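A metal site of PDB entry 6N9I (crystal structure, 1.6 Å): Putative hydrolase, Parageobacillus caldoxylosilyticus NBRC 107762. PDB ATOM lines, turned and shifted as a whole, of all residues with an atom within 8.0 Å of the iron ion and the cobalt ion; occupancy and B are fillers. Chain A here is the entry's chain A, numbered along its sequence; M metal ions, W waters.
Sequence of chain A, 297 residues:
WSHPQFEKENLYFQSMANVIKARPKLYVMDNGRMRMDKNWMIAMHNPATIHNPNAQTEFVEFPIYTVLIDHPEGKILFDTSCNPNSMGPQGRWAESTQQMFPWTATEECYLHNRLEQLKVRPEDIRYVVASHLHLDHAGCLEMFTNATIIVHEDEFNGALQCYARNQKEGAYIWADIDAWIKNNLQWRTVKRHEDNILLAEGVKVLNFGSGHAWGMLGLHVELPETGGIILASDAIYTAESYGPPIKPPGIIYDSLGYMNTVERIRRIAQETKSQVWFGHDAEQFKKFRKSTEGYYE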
ATOM      1  N   MET A  34      21.096  23.059  17.758  1.00  0.00           N
ATOM      2  CA  MET A  34      20.398  21.912  17.217  1.00  0.00           C
ATOM      3  C   MET A  34      20.954  21.635  15.813  1.00  0.00           C
ATOM      4  O   MET A  34      21.442  22.543  15.134  1.00  0.00           O
ATOM      5  CB  MET A  34      18.895  22.175  17.147  1.00  0.00           C
ATOM      6  CG  MET A  34      18.090  21.025  16.562  1.00  0.00           C
ATOM      7  SD  MET A  34      16.302  21.252  16.735  1.00  0.00           S
ATOM      8  CE  MET A  34      16.117  21.015  18.506  1.00  0.00           C
ATOM      9  N   MET A  36      20.042  19.294  12.079  1.00  0.00           N
ATOM     10  CA  MET A  36      19.060  18.541  11.323  1.00  0.00           C
ATOM     11  C   MET A  36      19.359  18.634   9.825  1.00  0.00           C
ATOM     12  O   MET A  36      20.181  19.444   9.383  1.00  0.00           O
ATOM     13  CB  MET A  36      17.643  19.062  11.579  1.00  0.00           C
ATOM     14  CG  MET A  36      17.370  20.387  10.907  1.00  0.00           C
ATOM     15  SD  MET A  36      15.760  21.071  11.376  1.00  0.00           S
ATOM     16  CE  MET A  36      15.794  22.594  10.441  1.00  0.00           C
ATOM     17  N   PHE A  62      22.305  25.025  13.918  1.00  0.00           N
ATOM     18  CA  PHE A  62      21.677  26.322  14.063  1.00  0.00           C
ATOM     19  C   PHE A  62      21.410  26.589  15.542  1.00  0.00           C
ATOM     20  O   PHE A  62      21.312  25.662  16.335  1.00  0.00           O
ATOM     21  CB  PHE A  62      20.391  26.404  13.225  1.00  0.00           C
ATOM     22  CG  PHE A  62      19.387  25.315  13.515  1.00  0.00           C
ATOM     23  CD1 PHE A  62      19.437  24.118  12.824  1.00  0.00           C
ATOM     24  CD2 PHE A  62      18.396  25.498  14.459  1.00  0.00           C
ATOM     25  CE1 PHE A  62      18.511  23.109  13.088  1.00  0.00           C
ATOM     26  CE2 PHE A  62      17.472  24.500  14.714  1.00  0.00           C
ATOM     27  CZ  PHE A  62      17.530  23.306  14.028  1.00  0.00           C
ATOM     28  N   PRO A  63      21.303  27.881  15.933  1.00  0.00           N
ATOM     29  CA  PRO A  63      21.077  28.235  17.327  1.00  0.00           C
ATOM     30  C   PRO A  63      19.613  28.136  17.771  1.00  0.00           C
ATOM     31  O   PRO A  63      18.701  28.428  16.997  1.00  0.00           O
ATOM     32  CB  PRO A  63      21.545  29.697  17.384  1.00  0.00           C
ATOM     33  CG  PRO A  63      21.271  30.236  15.991  1.00  0.00           C
ATOM     34  CD  PRO A  63      21.453  29.055  15.053  1.00  0.00           C
ATOM     35  N   ILE A  64      19.422  27.697  19.011  1.00  0.00           N
ATOM     36  CA  ILE A  64      18.162  27.789  19.730  1.00  0.00           C
ATOM     37  C   ILE A  64      18.284  28.944  20.727  1.00  0.00           C
ATOM     38  O   ILE A  64      19.172  28.931  21.570  1.00  0.00           O
ATOM     39  CB  ILE A  64      17.861  26.459  20.466  1.00  0.00           C
ATOM     40  CG1 ILE A  64      17.960  25.256  19.533  1.00  0.00           C
ATOM     41  CG2 ILE A  64      16.517  26.537  21.167  1.00  0.00           C
ATOM     42  CD1 ILE A  64      17.128  25.385  18.285  1.00  0.00           C
ATOM     43  N   ASP A  79       9.438  32.736  23.548  1.00  0.00           N
ATOM     44  CA  ASP A  79       9.913  31.361  23.335  1.00  0.00           C
ATOM     45  C   ASP A  79      10.615  30.855  24.609  1.00  0.00           C
ATOM     46  O   ASP A  79      10.905  31.642  25.513  1.00  0.00           O
ATOM     47  CB  ASP A  79      10.792  31.258  22.089  1.00  0.00           C
ATOM     48  CG  ASP A  79       9.994  31.092  20.802  1.00  0.00           C
ATOM     49  OD1 ASP A  79       8.769  30.883  20.900  1.00  0.00           O
ATOM     50  OD2 ASP A  79      10.613  31.160  19.716  1.00  0.00           O
ATOM     51  N   SER A 131       5.843  31.354  20.212  1.00  0.00           N
ATOM     52  CA  SER A 131       5.769  31.579  18.763  1.00  0.00           C
ATOM     53  C   SER A 131       5.022  30.410  18.118  1.00  0.00           C
ATOM     54  O   SER A 131       4.226  30.587  17.206  1.00  0.00           O
ATOM     55  CB  SER A 131       7.147  31.758  18.166  1.00  0.00           C
ATOM     56  OG  SER A 131       7.924  30.576  18.302  1.00  0.00           O
ATOM     57  N   HIS A 132       5.315  29.211  18.623  1.00  0.00           N
ATOM     58  CA  HIS A 132       4.607  27.974  18.293  1.00  0.00           C
ATOM     59  C   HIS A 132       5.036  26.916  19.311  1.00  0.00           C
ATOM     60  O   HIS A 132       5.769  27.231  20.228  1.00  0.00           O
ATOM     61  CB  HIS A 132       4.822  27.589  16.818  1.00  0.00           C
ATOM     62  CG  HIS A 132       6.238  27.326  16.419  1.00  0.00           C
ATOM     63  ND1 HIS A 132       7.259  28.217  16.690  1.00  0.00           N
ATOM     64  CD2 HIS A 132       6.789  26.306  15.727  1.00  0.00           C
ATOM     65  CE1 HIS A 132       8.394  27.736  16.202  1.00  0.00           C
ATOM     66  NE2 HIS A 132       8.129  26.565  15.599  1.00  0.00           N
ATOM     67  N   LEU A 133       4.561  25.663  19.162  1.00  0.00           N
ATOM     68  CA  LEU A 133       4.727  24.706  20.248  1.00  0.00           C
ATOM     69  C   LEU A 133       5.662  23.554  19.847  1.00  0.00           C
ATOM     70  O   LEU A 133       5.566  22.462  20.401  1.00  0.00           O
ATOM     71  CB  LEU A 133       3.356  24.194  20.679  1.00  0.00           C
ATOM     72  CG  LEU A 133       2.466  25.225  21.371  1.00  0.00           C
ATOM     73  CD1 LEU A 133       1.097  24.652  21.678  1.00  0.00           C
ATOM     74  CD2 LEU A 133       3.111  25.763  22.631  1.00  0.00           C
ATOM     75  N   HIS A 134       6.580  23.831  18.921  1.00  0.00           N
ATOM     76  CA  HIS A 134       7.616  22.864  18.540  1.00  0.00           C
ATOM     77  C   HIS A 134       8.563  22.623  19.708  1.00  0.00           C
ATOM     78  O   HIS A 134       8.677  23.436  20.622  1.00  0.00           O
ATOM     79  CB  HIS A 134       8.387  23.345  17.302  1.00  0.00           C
ATOM     80  CG  HIS A 134       7.735  22.979  16.006  1.00  0.00           C
ATOM     81  ND1 HIS A 134       8.159  23.504  14.802  1.00  0.00           N
ATOM     82  CD2 HIS A 134       6.701  22.156  15.720  1.00  0.00           C
ATOM     83  CE1 HIS A 134       7.408  23.024  13.824  1.00  0.00           C
ATOM     84  NE2 HIS A 134       6.512  22.192  14.371  1.00  0.00           N
ATOM     85  N   LEU A 135       9.286  21.494  19.637  1.00  0.00           N
ATOM     86  CA  LEU A 135      10.118  20.988  20.733  1.00  0.00           C
ATOM     87  C   LEU A 135      11.197  22.009  21.135  1.00  0.00           C
ATOM     88  O   LEU A 135      11.663  21.979  22.268  1.00  0.00           O
ATOM     89  CB  LEU A 135      10.729  19.653  20.312  1.00  0.00           C
ATOM     90  CG  LEU A 135      11.799  19.697  19.213  1.00  0.00           C
ATOM     91  CD1 LEU A 135      12.379  18.307  18.981  1.00  0.00           C
ATOM     92  CD2 LEU A 135      11.237  20.260  17.924  1.00  0.00           C
ATOM     93  N   ASP A 136      11.587  22.890  20.203  1.00  0.00           N
ATOM     94  CA  ASP A 136      12.704  23.803  20.430  1.00  0.00           C
ATOM     95  C   ASP A 136      12.213  25.216  20.780  1.00  0.00           C
ATOM     96  O   ASP A 136      13.006  26.152  20.829  1.00  0.00           O
ATOM     97  CB  ASP A 136      13.640  23.864  19.224  1.00  0.00           C
ATOM     98  CG  ASP A 136      12.920  24.101  17.902  1.00  0.00           C
ATOM     99  OD1 ASP A 136      11.856  23.506  17.701  1.00  0.00           O
ATOM    100  OD2 ASP A 136      13.444  24.894  17.094  1.00  0.00           O
ATOM    101  N   HIS A 137      10.909  25.364  21.049  1.00  0.00           N
ATOM    102  CA  HIS A 137      10.337  26.671  21.386  1.00  0.00           C
ATOM    103  C   HIS A 137       9.468  26.601  22.645  1.00  0.00           C
ATOM    104  O   HIS A 137       9.358  27.578  23.385  1.00  0.00           O
ATOM    105  CB  HIS A 137       9.548  27.243  20.192  1.00  0.00           C
ATOM    106  CG  HIS A 137      10.381  27.430  18.968  1.00  0.00           C
ATOM    107  ND1 HIS A 137      10.910  28.656  18.615  1.00  0.00           N
ATOM    108  CD2 HIS A 137      10.782  26.556  18.017  1.00  0.00           C
ATOM    109  CE1 HIS A 137      11.599  28.533  17.498  1.00  0.00           C
ATOM    110  NE2 HIS A 137      11.537  27.258  17.109  1.00  0.00           N
ATOM    111  N   GLU A 155      -2.463  26.435  17.032  1.00  0.00           N
ATOM    112  CA  GLU A 155      -1.240  25.738  17.421  1.00  0.00           C
ATOM    113  C   GLU A 155      -1.508  24.917  18.685  1.00  0.00           C
ATOM    114  O   GLU A 155      -1.124  23.751  18.789  1.00  0.00           O
ATOM    115  CB  GLU A 155      -0.107  26.748  17.632  1.00  0.00           C
ATOM    116  CG  GLU A 155       1.245  26.106  17.894  1.00  0.00           C
ATOM    117  CD  GLU A 155       1.863  25.416  16.693  1.00  0.00           C
ATOM    118  OE1 GLU A 155       1.279  25.521  15.588  1.00  0.00           O
ATOM    119  OE2 GLU A 155       2.928  24.783  16.858  1.00  0.00           O
ATOM    120  N   ALA A 171       7.546  16.734  15.998  1.00  0.00           N
ATOM    121  CA  ALA A 171       8.122  17.952  16.539  1.00  0.00           C
ATOM    122  C   ALA A 171       7.358  18.430  17.784  1.00  0.00           C
ATOM    123  O   ALA A 171       7.713  19.428  18.392  1.00  0.00           O
ATOM    124  CB  ALA A 171       8.141  19.024  15.473  1.00  0.00           C
ATOM    125  N   TYR A 172       6.293  17.703  18.139  1.00  0.00           N
ATOM    126  CA  TYR A 172       5.522  18.019  19.340  1.00  0.00           C
ATOM    127  C   TYR A 172       5.772  16.926  20.385  1.00  0.00           C
ATOM    128  O   TYR A 172       5.490  15.749  20.150  1.00  0.00           O
ATOM    129  CB  TYR A 172       4.047  18.215  18.997  1.00  0.00           C
ATOM    130  CG  TYR A 172       3.812  19.396  18.076  1.00  0.00           C
ATOM    131  CD1 TYR A 172       3.837  19.238  16.703  1.00  0.00           C
ATOM    132  CD2 TYR A 172       3.634  20.668  18.586  1.00  0.00           C
ATOM    133  CE1 TYR A 172       3.665  20.317  15.849  1.00  0.00           C
ATOM    134  CE2 TYR A 172       3.457  21.757  17.753  1.00  0.00           C
ATOM    135  CZ  TYR A 172       3.463  21.584  16.379  1.00  0.00           C
ATOM    136  OH  TYR A 172       3.291  22.654  15.547  1.00  0.00           O
ATOM    137  N   HIS A 212       4.406  27.861   8.710  1.00  0.00           N
ATOM    138  CA  HIS A 212       5.395  26.888   9.176  1.00  0.00           C
ATOM    139  C   HIS A 212       4.695  25.823  10.028  1.00  0.00           C
ATOM    140  O   HIS A 212       4.934  24.627   9.859  1.00  0.00           O
ATOM    141  CB  HIS A 212       6.531  27.590   9.930  1.00  0.00           C
ATOM    142  CG  HIS A 212       7.407  26.686  10.722  1.00  0.00           C
ATOM    143  ND1 HIS A 212       8.282  25.784  10.139  1.00  0.00           N
ATOM    144  CD2 HIS A 212       7.564  26.538  12.064  1.00  0.00           C
ATOM    145  CE1 HIS A 212       8.928  25.132  11.081  1.00  0.00           C
ATOM    146  NE2 HIS A 212       8.511  25.574  12.268  1.00  0.00           N
ATOM    147  N   ALA A 213       3.834  26.288  10.936  1.00  0.00           N
ATOM    148  CA  ALA A 213       3.070  25.438  11.837  1.00  0.00           C
ATOM    149  C   ALA A 213       1.592  25.866  11.798  1.00  0.00           C
ATOM    150  O   ALA A 213       1.202  26.680  10.972  1.00  0.00           O
ATOM    151  CB  ALA A 213       3.640  25.510  13.234  1.00  0.00           C
ATOM    152  N   MET A 216       1.317  30.610  14.153  1.00  0.00           N
ATOM    153  CA  MET A 216       2.560  31.284  14.475  1.00  0.00           C
ATOM    154  C   MET A 216       2.261  32.648  15.106  1.00  0.00           C
ATOM    155  O   MET A 216       1.387  33.379  14.621  1.00  0.00           O
ATOM    156  CB  MET A 216       3.418  31.496  13.221  1.00  0.00           C
ATOM    157  CG  MET A 216       3.683  30.215  12.433  1.00  0.00           C
ATOM    158  SD  MET A 216       4.645  29.014  13.372  1.00  0.00           S
ATOM    159  CE  MET A 216       6.216  29.859  13.547  1.00  0.00           C
ATOM    160  N   SER A 233      10.613  34.339  14.759  1.00  0.00           N
ATOM    161  CA  SER A 233      10.751  32.926  15.076  1.00  0.00           C
ATOM    162  C   SER A 233      10.772  32.128  13.762  1.00  0.00           C
ATOM    163  O   SER A 233      11.391  32.558  12.780  1.00  0.00           O
ATOM    164  CB  SER A 233       9.656  32.456  15.992  1.00  0.00           C
ATOM    165  OG  SER A 233       9.891  31.121  16.425  1.00  0.00           O
ATOM    166  N   ASP A 234      10.079  30.992  13.735  1.00  0.00           N
ATOM    167  CA  ASP A 234      10.209  30.043  12.630  1.00  0.00           C
ATOM    168  C   ASP A 234       9.288  30.426  11.467  1.00  0.00           C
ATOM    169  O   ASP A 234       9.147  29.675  10.506  1.00  0.00           O
ATOM    170  CB  ASP A 234       9.973  28.614  13.090  1.00  0.00           C
ATOM    171  CG  ASP A 234      11.132  28.048  13.889  1.00  0.00           C
ATOM    172  OD1 ASP A 234      12.117  28.809  14.091  1.00  0.00           O
ATOM    173  OD2 ASP A 234      11.058  26.876  14.296  1.00  0.00           O
ATOM    174  N   ALA A 235       8.682  31.619  11.535  1.00  0.00           N
ATOM    175  CA  ALA A 235       8.016  32.174  10.370  1.00  0.00           C
ATOM    176  C   ALA A 235       9.072  32.433   9.281  1.00  0.00           C
ATOM    177  O   ALA A 235       8.775  32.391   8.094  1.00  0.00           O
ATOM    178  CB  ALA A 235       7.284  33.441  10.744  1.00  0.00           C
ATOM    179  N   TYR A 237      13.102  31.094   9.059  1.00  0.00           N
ATOM    180  CA  TYR A 237      14.211  30.363   9.657  1.00  0.00           C
ATOM    181  C   TYR A 237      15.495  31.206   9.628  1.00  0.00           C
ATOM    182  O   TYR A 237      16.157  31.366  10.652  1.00  0.00           O
ATOM    183  CB  TYR A 237      14.446  29.056   8.908  1.00  0.00           C
ATOM    184  CG  TYR A 237      13.691  27.844   9.427  1.00  0.00           C
ATOM    185  CD1 TYR A 237      13.305  27.724  10.749  1.00  0.00           C
ATOM    186  CD2 TYR A 237      13.431  26.779   8.576  1.00  0.00           C
ATOM    187  CE1 TYR A 237      12.649  26.596  11.208  1.00  0.00           C
ATOM    188  CE2 TYR A 237      12.775  25.640   9.022  1.00  0.00           C
ATOM    189  CZ  TYR A 237      12.381  25.549  10.342  1.00  0.00           C
ATOM    190  OH  TYR A 237      11.741  24.412  10.763  1.00  0.00           O
ATOM    191  N   ILE A 251       9.964  21.697   6.700  1.00  0.00           N
ATOM    192  CA  ILE A 251       9.014  21.655   7.805  1.00  0.00           C
ATOM    193  C   ILE A 251       7.990  22.775   7.602  1.00  0.00           C
ATOM    194  O   ILE A 251       8.270  23.944   7.882  1.00  0.00           O
ATOM    195  CB  ILE A 251       9.718  21.791   9.173  1.00  0.00           C
ATOM    196  CG1 ILE A 251      10.767  20.700   9.382  1.00  0.00           C
ATOM    197  CG2 ILE A 251       8.694  21.793  10.294  1.00  0.00           C
ATOM    198  CD1 ILE A 251      11.387  20.700  10.757  1.00  0.00           C
ATOM    199  N   GLY A 279      14.458  32.942  13.170  1.00  0.00           N
ATOM    200  CA  GLY A 279      14.300  31.878  14.161  1.00  0.00           C
ATOM    201  C   GLY A 279      15.610  31.167  14.462  1.00  0.00           C
ATOM    202  O   GLY A 279      15.907  30.885  15.620  1.00  0.00           O
ATOM    203  N   HIS A 280      16.392  30.867  13.423  1.00  0.00           N
ATOM    204  CA  HIS A 280      17.538  29.972  13.556  1.00  0.00           C
ATOM    205  C   HIS A 280      18.640  30.333  12.552  1.00  0.00           C
ATOM    206  O   HIS A 280      19.131  29.461  11.824  1.00  0.00           O
ATOM    207  CB  HIS A 280      17.101  28.517  13.354  1.00  0.00           C
ATOM    208  CG  HIS A 280      16.062  28.045  14.317  1.00  0.00           C
ATOM    209  ND1 HIS A 280      16.307  27.942  15.671  1.00  0.00           N
ATOM    210  CD2 HIS A 280      14.804  27.606  14.125  1.00  0.00           C
ATOM    211  CE1 HIS A 280      15.235  27.484  16.282  1.00  0.00           C
ATOM    212  NE2 HIS A 280      14.294  27.267  15.350  1.00  0.00           N
HETATM  213 FE    FE M   1      12.350  26.005  15.495  1.00  0.00          FE
HETATM  214 CO    CO M   2       9.353  25.144  14.384  1.00  0.00          CO
HETATM  215  O   HOH W   1      12.888  24.518  13.960  1.00  0.00           O
HETATM  216  O   HOH W   2      10.742  24.685  15.610  1.00  0.00           O
HETATM  217  O   HOH W   3      10.716  23.891  13.366  1.00  0.00           O
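A ring nitrogen (ND1) of His 132 sits at hydrogen-bond distance from the side-chain hydroxyl of Ser 131, at 2.9 Å. The backbone carbonyl oxygen (O) of Ile 251 is in hydrogen-bond range of a ring nitrogen (ND1) of His 212 (2.9 Å). N of His 280 sits at hydrogen-bond distance from O of Tyr 237 (2.8 Å). The backbone carbonyl oxygen (O) of Pro 63 is in hydrogen-bond range of a ring nitrogen (ND1) of His 280 (2.8 Å). A ring nitrogen (NE2) of His 134 lies close to the side-chain hydroxyl (OH) of Tyr 172 (3.5 Å). ND1 of His 137 lies within hydrogen-bond range of OD2 of Asp 79. A ring nitrogen (ND1) of His 137 sits close to the side-chain hydroxyl (OG) of Ser 233, at 3.5 Å.
Four residues have an atom within 4 Å of the iron ion: Asp 136, His 137, Asp 234 and His 280. The nearest printed residue that does not touch the iron ion is His 132 (4.3 Å).
The cobalt ion is bound by water W2 (1.9 Å), a ring nitrogen (ND1) of His 134 (2.1 Å), water W3 (2.1 Å), a ring nitrogen (NE2) of His 132 (2.2 Å), a ring nitrogen (NE2) of His 212 (2.3 Å) and the side-chain carboxylate (OD2) of Asp 234 (2.4 Å).
Within 4 Å of the cobalt ion: His 132, His 134, His 212 and Asp 234.
OD2 of Asp 234 is bound to the iron ion (2.0 Å). Water W2 binds the iron ion. A ring nitrogen (NE2) of His 137 binds the iron ion, at 2.2 Å. The iron ion is bound by water W1. The side-chain carboxylate (OD2) of Asp 136 is bound to the iron ion (2.2 Å). A ring nitrogen (NE2) of His 280 binds the iron ion, at 2.3 Å.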
